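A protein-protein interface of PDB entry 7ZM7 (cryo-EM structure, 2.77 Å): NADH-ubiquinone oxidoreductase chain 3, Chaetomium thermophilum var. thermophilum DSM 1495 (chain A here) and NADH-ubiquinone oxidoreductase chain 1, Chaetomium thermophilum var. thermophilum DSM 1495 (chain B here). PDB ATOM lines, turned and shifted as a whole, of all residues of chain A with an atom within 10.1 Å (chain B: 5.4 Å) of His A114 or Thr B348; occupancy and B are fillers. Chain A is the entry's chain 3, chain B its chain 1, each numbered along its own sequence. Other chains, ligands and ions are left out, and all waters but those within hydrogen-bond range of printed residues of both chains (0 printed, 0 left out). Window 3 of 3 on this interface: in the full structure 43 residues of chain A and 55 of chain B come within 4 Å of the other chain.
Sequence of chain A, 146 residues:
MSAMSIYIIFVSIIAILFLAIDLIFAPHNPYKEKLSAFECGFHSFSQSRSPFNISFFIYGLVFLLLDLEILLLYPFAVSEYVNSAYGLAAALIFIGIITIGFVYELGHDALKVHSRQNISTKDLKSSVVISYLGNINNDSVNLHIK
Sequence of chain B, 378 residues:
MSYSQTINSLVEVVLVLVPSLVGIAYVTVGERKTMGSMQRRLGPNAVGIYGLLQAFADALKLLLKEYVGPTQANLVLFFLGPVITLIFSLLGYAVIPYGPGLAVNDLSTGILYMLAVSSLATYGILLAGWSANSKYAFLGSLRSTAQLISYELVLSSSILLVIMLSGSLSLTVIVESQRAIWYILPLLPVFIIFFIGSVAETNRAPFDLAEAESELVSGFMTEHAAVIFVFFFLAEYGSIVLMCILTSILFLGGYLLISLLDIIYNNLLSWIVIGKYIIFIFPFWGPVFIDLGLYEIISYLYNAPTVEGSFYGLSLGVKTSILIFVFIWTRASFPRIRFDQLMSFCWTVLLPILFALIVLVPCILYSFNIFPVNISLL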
ATOM      1  N   SER A  55     -19.196  -5.765   4.625  1.00  0.00           N
ATOM      2  CA  SER A  55     -20.232  -6.377   3.806  1.00  0.00           C
ATOM      3  C   SER A  55     -20.318  -5.740   2.427  1.00  0.00           C
ATOM      4  O   SER A  55     -20.761  -6.388   1.476  1.00  0.00           O
ATOM      5  CB  SER A  55     -21.576  -6.302   4.531  1.00  0.00           C
ATOM      6  OG  SER A  55     -21.978  -4.969   4.732  1.00  0.00           O
ATOM      7  N   TYR A  59     -20.520  -7.982  -1.026  1.00  0.00           N
ATOM      8  CA  TYR A  59     -21.523  -7.836  -2.073  1.00  0.00           C
ATOM      9  C   TYR A  59     -20.878  -7.829  -3.449  1.00  0.00           C
ATOM     10  O   TYR A  59     -21.332  -8.524  -4.361  1.00  0.00           O
ATOM     11  CB  TYR A  59     -22.329  -6.557  -1.844  1.00  0.00           C
ATOM     12  CG  TYR A  59     -23.193  -6.620  -0.622  1.00  0.00           C
ATOM     13  CD1 TYR A  59     -23.575  -7.827  -0.098  1.00  0.00           C
ATOM     14  CD2 TYR A  59     -23.546  -5.470   0.068  1.00  0.00           C
ATOM     15  CE1 TYR A  59     -24.339  -7.898   1.026  1.00  0.00           C
ATOM     16  CE2 TYR A  59     -24.304  -5.536   1.206  1.00  0.00           C
ATOM     17  CZ  TYR A  59     -24.698  -6.756   1.673  1.00  0.00           C
ATOM     18  OH  TYR A  59     -25.458  -6.850   2.809  1.00  0.00           O
ATOM     19  N   VAL A  62     -19.106 -11.551  -4.136  1.00  0.00           N
ATOM     20  CA  VAL A  62     -19.983 -12.672  -4.413  1.00  0.00           C
ATOM     21  C   VAL A  62     -20.696 -12.460  -5.728  1.00  0.00           C
ATOM     22  O   VAL A  62     -20.950 -13.415  -6.463  1.00  0.00           O
ATOM     23  CB  VAL A  62     -20.958 -12.879  -3.251  1.00  0.00           C
ATOM     24  CG1 VAL A  62     -21.824 -14.068  -3.531  1.00  0.00           C
ATOM     25  CG2 VAL A  62     -20.177 -13.093  -1.993  1.00  0.00           C
ATOM     26  N   PHE A 102     -21.311 -21.783  -3.065  1.00  0.00           N
ATOM     27  CA  PHE A 102     -22.434 -20.962  -2.663  1.00  0.00           C
ATOM     28  C   PHE A 102     -23.025 -21.399  -1.332  1.00  0.00           C
ATOM     29  O   PHE A 102     -23.505 -20.554  -0.573  1.00  0.00           O
ATOM     30  CB  PHE A 102     -23.501 -20.996  -3.756  1.00  0.00           C
ATOM     31  CG  PHE A 102     -24.743 -20.245  -3.413  1.00  0.00           C
ATOM     32  CD1 PHE A 102     -24.696 -18.888  -3.187  1.00  0.00           C
ATOM     33  CD2 PHE A 102     -25.961 -20.895  -3.306  1.00  0.00           C
ATOM     34  CE1 PHE A 102     -25.829 -18.193  -2.868  1.00  0.00           C
ATOM     35  CE2 PHE A 102     -27.086 -20.201  -2.990  1.00  0.00           C
ATOM     36  CZ  PHE A 102     -27.021 -18.842  -2.774  1.00  0.00           C
ATOM     37  N   VAL A 103     -23.007 -22.694  -1.016  1.00  0.00           N
ATOM     38  CA  VAL A 103     -23.490 -23.114   0.292  1.00  0.00           C
ATOM     39  C   VAL A 103     -22.485 -22.789   1.381  1.00  0.00           C
ATOM     40  O   VAL A 103     -22.826 -22.827   2.565  1.00  0.00           O
ATOM     41  CB  VAL A 103     -23.838 -24.617   0.318  1.00  0.00           C
ATOM     42  CG1 VAL A 103     -24.714 -24.968  -0.844  1.00  0.00           C
ATOM     43  CG2 VAL A 103     -22.617 -25.461   0.347  1.00  0.00           C
ATOM     44  N   GLU A 105     -20.880 -19.702   1.571  1.00  0.00           N
ATOM     45  CA  GLU A 105     -21.256 -18.371   2.028  1.00  0.00           C
ATOM     46  C   GLU A 105     -22.643 -18.359   2.650  1.00  0.00           C
ATOM     47  O   GLU A 105     -22.932 -17.512   3.498  1.00  0.00           O
ATOM     48  CB  GLU A 105     -21.180 -17.377   0.885  1.00  0.00           C
ATOM     49  CG  GLU A 105     -22.039 -17.715  -0.281  1.00  0.00           C
ATOM     50  CD  GLU A 105     -21.681 -16.884  -1.487  1.00  0.00           C
ATOM     51  OE1 GLU A 105     -20.849 -15.977  -1.318  1.00  0.00           O
ATOM     52  OE2 GLU A 105     -22.212 -17.138  -2.593  1.00  0.00           O
ATOM     53  N   LEU A 106     -23.517 -19.273   2.244  1.00  0.00           N
ATOM     54  CA  LEU A 106     -24.767 -19.435   2.967  1.00  0.00           C
ATOM     55  C   LEU A 106     -24.519 -19.973   4.362  1.00  0.00           C
ATOM     56  O   LEU A 106     -25.192 -19.579   5.317  1.00  0.00           O
ATOM     57  CB  LEU A 106     -25.702 -20.356   2.202  1.00  0.00           C
ATOM     58  CG  LEU A 106     -26.488 -19.682   1.099  1.00  0.00           C
ATOM     59  CD1 LEU A 106     -27.640 -20.574   0.700  1.00  0.00           C
ATOM     60  CD2 LEU A 106     -26.972 -18.313   1.545  1.00  0.00           C
ATOM     61  N   GLY A 107     -23.539 -20.865   4.494  1.00  0.00           N
ATOM     62  CA  GLY A 107     -23.284 -21.494   5.770  1.00  0.00           C
ATOM     63  C   GLY A 107     -22.541 -20.598   6.736  1.00  0.00           C
ATOM     64  O   GLY A 107     -22.498 -20.873   7.936  1.00  0.00           O
ATOM     65  N   HIS A 108     -21.937 -19.532   6.238  1.00  0.00           N
ATOM     66  CA  HIS A 108     -21.110 -18.680   7.077  1.00  0.00           C
ATOM     67  C   HIS A 108     -21.652 -17.268   7.228  1.00  0.00           C
ATOM     68  O   HIS A 108     -21.052 -16.472   7.956  1.00  0.00           O
ATOM     69  CB  HIS A 108     -19.688 -18.614   6.529  1.00  0.00           C
ATOM     70  CG  HIS A 108     -18.883 -19.843   6.794  1.00  0.00           C
ATOM     71  ND1 HIS A 108     -17.530 -19.808   7.033  1.00  0.00           N
ATOM     72  CD2 HIS A 108     -19.238 -21.146   6.842  1.00  0.00           C
ATOM     73  CE1 HIS A 108     -17.090 -21.035   7.230  1.00  0.00           C
ATOM     74  NE2 HIS A 108     -18.107 -21.864   7.119  1.00  0.00           N
ATOM     75  N   ASP A 109     -22.755 -16.941   6.560  1.00  0.00           N
ATOM     76  CA  ASP A 109     -23.273 -15.585   6.533  1.00  0.00           C
ATOM     77  C   ASP A 109     -22.176 -14.598   6.155  1.00  0.00           C
ATOM     78  O   ASP A 109     -21.937 -13.600   6.836  1.00  0.00           O
ATOM     79  CB  ASP A 109     -23.901 -15.215   7.871  1.00  0.00           C
ATOM     80  CG  ASP A 109     -24.667 -13.914   7.814  1.00  0.00           C
ATOM     81  OD1 ASP A 109     -25.134 -13.536   6.715  1.00  0.00           O
ATOM     82  OD2 ASP A 109     -24.753 -13.240   8.862  1.00  0.00           O
ATOM     83  N   ALA A 110     -21.461 -14.905   5.080  1.00  0.00           N
ATOM     84  CA  ALA A 110     -20.427 -13.982   4.648  1.00  0.00           C
ATOM     85  C   ALA A 110     -21.041 -12.661   4.237  1.00  0.00           C
ATOM     86  O   ALA A 110     -20.478 -11.593   4.506  1.00  0.00           O
ATOM     87  CB  ALA A 110     -19.622 -14.591   3.508  1.00  0.00           C
ATOM     88  N   LEU A 111     -22.215 -12.719   3.615  1.00  0.00           N
ATOM     89  CA  LEU A 111     -22.942 -11.522   3.258  1.00  0.00           C
ATOM     90  C   LEU A 111     -23.320 -10.754   4.515  1.00  0.00           C
ATOM     91  O   LEU A 111     -23.685  -9.575   4.437  1.00  0.00           O
ATOM     92  CB  LEU A 111     -24.187 -11.911   2.454  1.00  0.00           C
ATOM     93  CG  LEU A 111     -24.142 -12.245   0.937  1.00  0.00           C
ATOM     94  CD1 LEU A 111     -23.715 -11.123   0.037  1.00  0.00           C
ATOM     95  CD2 LEU A 111     -23.308 -13.485   0.642  1.00  0.00           C
ATOM     96  N   LYS A 112     -23.232 -11.413   5.674  1.00  0.00           N
ATOM     97  CA  LYS A 112     -23.520 -10.821   6.977  1.00  0.00           C
ATOM     98  C   LYS A 112     -24.890 -10.176   6.952  1.00  0.00           C
ATOM     99  O   LYS A 112     -25.092  -9.034   7.367  1.00  0.00           O
ATOM    100  CB  LYS A 112     -22.418  -9.858   7.410  1.00  0.00           C
ATOM    101  CG  LYS A 112     -21.205 -10.650   7.811  1.00  0.00           C
ATOM    102  CD  LYS A 112     -20.177  -9.903   8.571  1.00  0.00           C
ATOM    103  CE  LYS A 112     -19.117 -10.889   9.037  1.00  0.00           C
ATOM    104  NZ  LYS A 112     -19.562 -11.694  10.199  1.00  0.00           N
ATOM    105  N   VAL A 113     -25.832 -10.942   6.434  1.00  0.00           N
ATOM    106  CA  VAL A 113     -27.210 -10.520   6.292  1.00  0.00           C
ATOM    107  C   VAL A 113     -28.059 -11.031   7.447  1.00  0.00           C
ATOM    108  O   VAL A 113     -28.933 -10.321   7.950  1.00  0.00           O
ATOM    109  CB  VAL A 113     -27.725 -11.021   4.933  1.00  0.00           C
ATOM    110  CG1 VAL A 113     -29.131 -10.800   4.845  1.00  0.00           C
ATOM    111  CG2 VAL A 113     -27.057 -10.286   3.805  1.00  0.00           C
ATOM    112  N   HIS A 114     -27.802 -12.257   7.889  1.00  0.00           N
ATOM    113  CA  HIS A 114     -28.512 -12.832   9.022  1.00  0.00           C
ATOM    114  C   HIS A 114     -27.913 -12.279  10.311  1.00  0.00           C
ATOM    115  O   HIS A 114     -27.141 -11.316  10.302  1.00  0.00           O
ATOM    116  CB  HIS A 114     -28.451 -14.355   8.962  1.00  0.00           C
ATOM    117  CG  HIS A 114     -29.497 -14.965   8.083  1.00  0.00           C
ATOM    118  ND1 HIS A 114     -30.131 -16.148   8.393  1.00  0.00           N
ATOM    119  CD2 HIS A 114     -30.016 -14.558   6.901  1.00  0.00           C
ATOM    120  CE1 HIS A 114     -30.999 -16.443   7.441  1.00  0.00           C
ATOM    121  NE2 HIS A 114     -30.948 -15.495   6.523  1.00  0.00           N
ATOM    122  N   SER A 115     -28.269 -12.885  11.444  1.00  0.00           N
ATOM    123  CA  SER A 115     -27.772 -12.476  12.756  1.00  0.00           C
ATOM    124  C   SER A 115     -28.118 -11.012  13.040  1.00  0.00           C
ATOM    125  O   SER A 115     -27.249 -10.149  13.173  1.00  0.00           O
ATOM    126  CB  SER A 115     -26.264 -12.716  12.872  1.00  0.00           C
ATOM    127  OG  SER A 115     -25.538 -11.707  12.191  1.00  0.00           O
ATOM    128  N   ARG A 116     -29.417 -10.748  13.125  1.00  0.00           N
ATOM    129  CA  ARG A 116     -29.898  -9.401  13.398  1.00  0.00           C
ATOM    130  C   ARG A 116     -30.858  -9.391  14.581  1.00  0.00           C
ATOM    131  O   ARG A 116     -30.497  -8.980  15.682  1.00  0.00           O
ATOM    132  CB  ARG A 116     -30.579  -8.815  12.164  1.00  0.00           C
ATOM    133  CG  ARG A 116     -30.941  -7.349  12.300  1.00  0.00           C
ATOM    134  CD  ARG A 116     -29.718  -6.469  12.131  1.00  0.00           C
ATOM    135  NE  ARG A 116     -29.057  -6.201  13.403  1.00  0.00           N
ATOM    136  CZ  ARG A 116     -27.829  -5.708  13.515  1.00  0.00           C
ATOM    137  NH1 ARG A 116     -27.306  -5.494  14.714  1.00  0.00           N
ATOM    138  NH2 ARG A 116     -27.124  -5.428  12.428  1.00  0.00           N
ATOM    139  N   MET B 343     -31.571  -8.083   0.933  1.00  0.00           N
ATOM    140  CA  MET B 343     -30.337  -8.835   0.633  1.00  0.00           C
ATOM    141  C   MET B 343     -30.550 -10.304   0.991  1.00  0.00           C
ATOM    142  O   MET B 343     -30.080 -11.163   0.241  1.00  0.00           O
ATOM    143  CB  MET B 343     -29.132  -8.242   1.364  1.00  0.00           C
ATOM    144  CG  MET B 343     -28.704  -6.883   0.856  1.00  0.00           C
ATOM    145  SD  MET B 343     -28.588  -6.714  -0.942  1.00  0.00           S
ATOM    146  CE  MET B 343     -26.944  -7.342  -1.263  1.00  0.00           C
ATOM    147  N   SER B 344     -31.233 -10.570   2.099  1.00  0.00           N
ATOM    148  CA  SER B 344     -31.504 -11.966   2.506  1.00  0.00           C
ATOM    149  C   SER B 344     -32.462 -12.594   1.499  1.00  0.00           C
ATOM    150  O   SER B 344     -32.283 -13.768   1.172  1.00  0.00           O
ATOM    151  CB  SER B 344     -32.051 -12.018   3.894  1.00  0.00           C
ATOM    152  OG  SER B 344     -33.442 -11.747   3.912  1.00  0.00           O
ATOM    153  N   PHE B 345     -33.433 -11.821   1.024  1.00  0.00           N
ATOM    154  CA  PHE B 345     -34.371 -12.335   0.044  1.00  0.00           C
ATOM    155  C   PHE B 345     -33.655 -12.782  -1.221  1.00  0.00           C
ATOM    156  O   PHE B 345     -33.930 -13.857  -1.752  1.00  0.00           O
ATOM    157  CB  PHE B 345     -35.413 -11.257  -0.253  1.00  0.00           C
ATOM    158  CG  PHE B 345     -36.539 -11.726  -1.106  1.00  0.00           C
ATOM    159  CD1 PHE B 345     -37.141 -12.943  -0.871  1.00  0.00           C
ATOM    160  CD2 PHE B 345     -36.994 -10.955  -2.146  1.00  0.00           C
ATOM    161  CE1 PHE B 345     -38.159 -13.370  -1.654  1.00  0.00           C
ATOM    162  CE2 PHE B 345     -38.019 -11.394  -2.934  1.00  0.00           C
ATOM    163  CZ  PHE B 345     -38.605 -12.596  -2.679  1.00  0.00           C
ATOM    164  N   CYS B 346     -32.707 -11.982  -1.691  1.00  0.00           N
ATOM    165  CA  CYS B 346     -32.008 -12.287  -2.927  1.00  0.00           C
ATOM    166  C   CYS B 346     -31.077 -13.479  -2.755  1.00  0.00           C
ATOM    167  O   CYS B 346     -31.078 -14.404  -3.571  1.00  0.00           O
ATOM    168  CB  CYS B 346     -31.229 -11.054  -3.378  1.00  0.00           C
ATOM    169  SG  CYS B 346     -30.225 -11.286  -4.809  1.00  0.00           S
ATOM    170  N   TRP B 347     -30.293 -13.476  -1.680  1.00  0.00           N
ATOM    171  CA  TRP B 347     -29.148 -14.357  -1.536  1.00  0.00           C
ATOM    172  C   TRP B 347     -29.462 -15.657  -0.833  1.00  0.00           C
ATOM    173  O   TRP B 347     -28.766 -16.647  -1.059  1.00  0.00           O
ATOM    174  CB  TRP B 347     -28.038 -13.628  -0.780  1.00  0.00           C
ATOM    175  CG  TRP B 347     -27.370 -12.639  -1.638  1.00  0.00           C
ATOM    176  CD1 TRP B 347     -27.506 -11.297  -1.591  1.00  0.00           C
ATOM    177  CD2 TRP B 347     -26.481 -12.919  -2.705  1.00  0.00           C
ATOM    178  NE1 TRP B 347     -26.745 -10.716  -2.552  1.00  0.00           N
ATOM    179  CE2 TRP B 347     -26.101 -11.696  -3.256  1.00  0.00           C
ATOM    180  CE3 TRP B 347     -25.954 -14.096  -3.240  1.00  0.00           C
ATOM    181  CZ2 TRP B 347     -25.225 -11.604  -4.322  1.00  0.00           C
ATOM    182  CZ3 TRP B 347     -25.098 -14.006  -4.297  1.00  0.00           C
ATOM    183  CH2 TRP B 347     -24.736 -12.770  -4.828  1.00  0.00           C
ATOM    184  N   THR B 348     -30.471 -15.686   0.025  1.00  0.00           N
ATOM    185  CA  THR B 348     -30.780 -16.895   0.766  1.00  0.00           C
ATOM    186  C   THR B 348     -32.141 -17.487   0.431  1.00  0.00           C
ATOM    187  O   THR B 348     -32.448 -18.583   0.904  1.00  0.00           O
ATOM    188  CB  THR B 348     -30.677 -16.635   2.272  1.00  0.00           C
ATOM    189  OG1 THR B 348     -31.861 -15.991   2.739  1.00  0.00           O
ATOM    190  CG2 THR B 348     -29.498 -15.751   2.567  1.00  0.00           C
ATOM    191  N   VAL B 349     -32.943 -16.821  -0.392  1.00  0.00           N
ATOM    192  CA  VAL B 349     -34.198 -17.396  -0.862  1.00  0.00           C
ATOM    193  C   VAL B 349     -34.191 -17.539  -2.379  1.00  0.00           C
ATOM    194  O   VAL B 349     -34.240 -18.651  -2.905  1.00  0.00           O
ATOM    195  CB  VAL B 349     -35.411 -16.561  -0.405  1.00  0.00           C
ATOM    196  CG1 VAL B 349     -36.680 -17.088  -1.041  1.00  0.00           C
ATOM    197  CG2 VAL B 349     -35.521 -16.552   1.091  1.00  0.00           C
ATOM    198  N   LEU B 350     -34.105 -16.417  -3.092  1.00  0.00           N
ATOM    199  CA  LEU B 350     -34.342 -16.406  -4.534  1.00  0.00           C
ATOM    200  C   LEU B 350     -33.256 -17.153  -5.295  1.00  0.00           C
ATOM    201  O   LEU B 350     -33.539 -18.085  -6.050  1.00  0.00           O
ATOM    202  CB  LEU B 350     -34.435 -14.964  -5.031  1.00  0.00           C
ATOM    203  CG  LEU B 350     -35.693 -14.141  -4.757  1.00  0.00           C
ATOM    204  CD1 LEU B 350     -35.505 -12.760  -5.321  1.00  0.00           C
ATOM    205  CD2 LEU B 350     -36.889 -14.797  -5.367  1.00  0.00           C
ATOM    206  N   PRO B 352     -30.952 -19.345  -4.290  1.00  0.00           N
ATOM    207  CA  PRO B 352     -30.969 -20.796  -4.095  1.00  0.00           C
ATOM    208  C   PRO B 352     -32.020 -21.506  -4.916  1.00  0.00           C
ATOM    209  O   PRO B 352     -31.736 -22.558  -5.488  1.00  0.00           O
ATOM    210  CB  PRO B 352     -31.225 -20.926  -2.590  1.00  0.00           C
ATOM    211  CG  PRO B 352     -30.612 -19.760  -2.045  1.00  0.00           C
ATOM    212  CD  PRO B 352     -30.898 -18.655  -2.995  1.00  0.00           C
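The side-chain carboxylate (OD1) of Asp A109 sits at hydrogen-bond distance from the backbone NH (N) of Val A113 (2.7 Å).
The backbone carbonyl oxygen (O) of Ser B344 is in hydrogen-bond range of the side-chain hydroxyl (OG1) of Thr B348.
The backbone carbonyl oxygen of Ser B344 is in hydrogen-bond range of the backbone NH of Val B349, at 3.5 Å.
The side-chain carboxylate of Asp A109 sits at hydrogen-bond distance from the backbone NH of His A114 (3.2 Å).
Printed residues of chain B within 4 Å of His A114: Thr B348.
Thr B348 touches just these residues of chain A: Leu A106 and His A114.
No residue of chain A comes within 4 Å of Val B349.
Printed residues of chain B within 4 Å of Leu A106: Trp B347 and Thr B348.
Printed residues of chain B within 4 Å of Phe A102: Trp B347 (3.3 Å) and Pro B352 (3.7 Å).
Of the printed residues of chain A, Met B343 touches Tyr A59 (3.5 Å) and Val A113 (3.8 Å).
Val A103 touches none of the printed residues of chain B.
The nearest residue of chain B that does not touch His A114 is Ser B344 (4.4 Å).
The nearest printed residue of chain A that does not touch Thr B348 is Phe A102 (5.4 Å).
Tyr A59 touches Met B343.
CG1 of Val A62 touches CZ3 of Trp B347, at 3.4 Å.
O of Trp B347 touches CZ of Phe A102, at 3.3 Å.
Pro B352 touches Phe A102 (CG to CE2, 3.7 Å).
Trp B347 touches Leu A106.
Leu A106 touches Thr B348 (CD2 to CG2, 3.7 Å).
Val A113 touches Met B343 (CG2 to CB, 3.8 Å).
Val A113 touches Ser B344 (CG1 to CB, 3.3 Å).
His A114 touches Thr B348 (NE2 to OG1, 3.9 Å).
Of the 17 printed residues of chain A, 6 touch a printed residue of chain B.
Hydrophobic or aromatic side chains of chain A within 4 Å of the printed part of chain B: Tyr A59, Val A62, Phe A102, Leu A106, Val A113 and His A114.
Printed residues of chain B that touch a printed residue of chain A: Met B343, Ser B344, Trp B347, Thr B348 and Pro B352.
Hydrophobic or aromatic side chains of chain B within 4 Å of the printed part of chain A: Met B343, Trp B347 and Pro B352.
Among the printed residues, 9 pairs touch across the chains.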
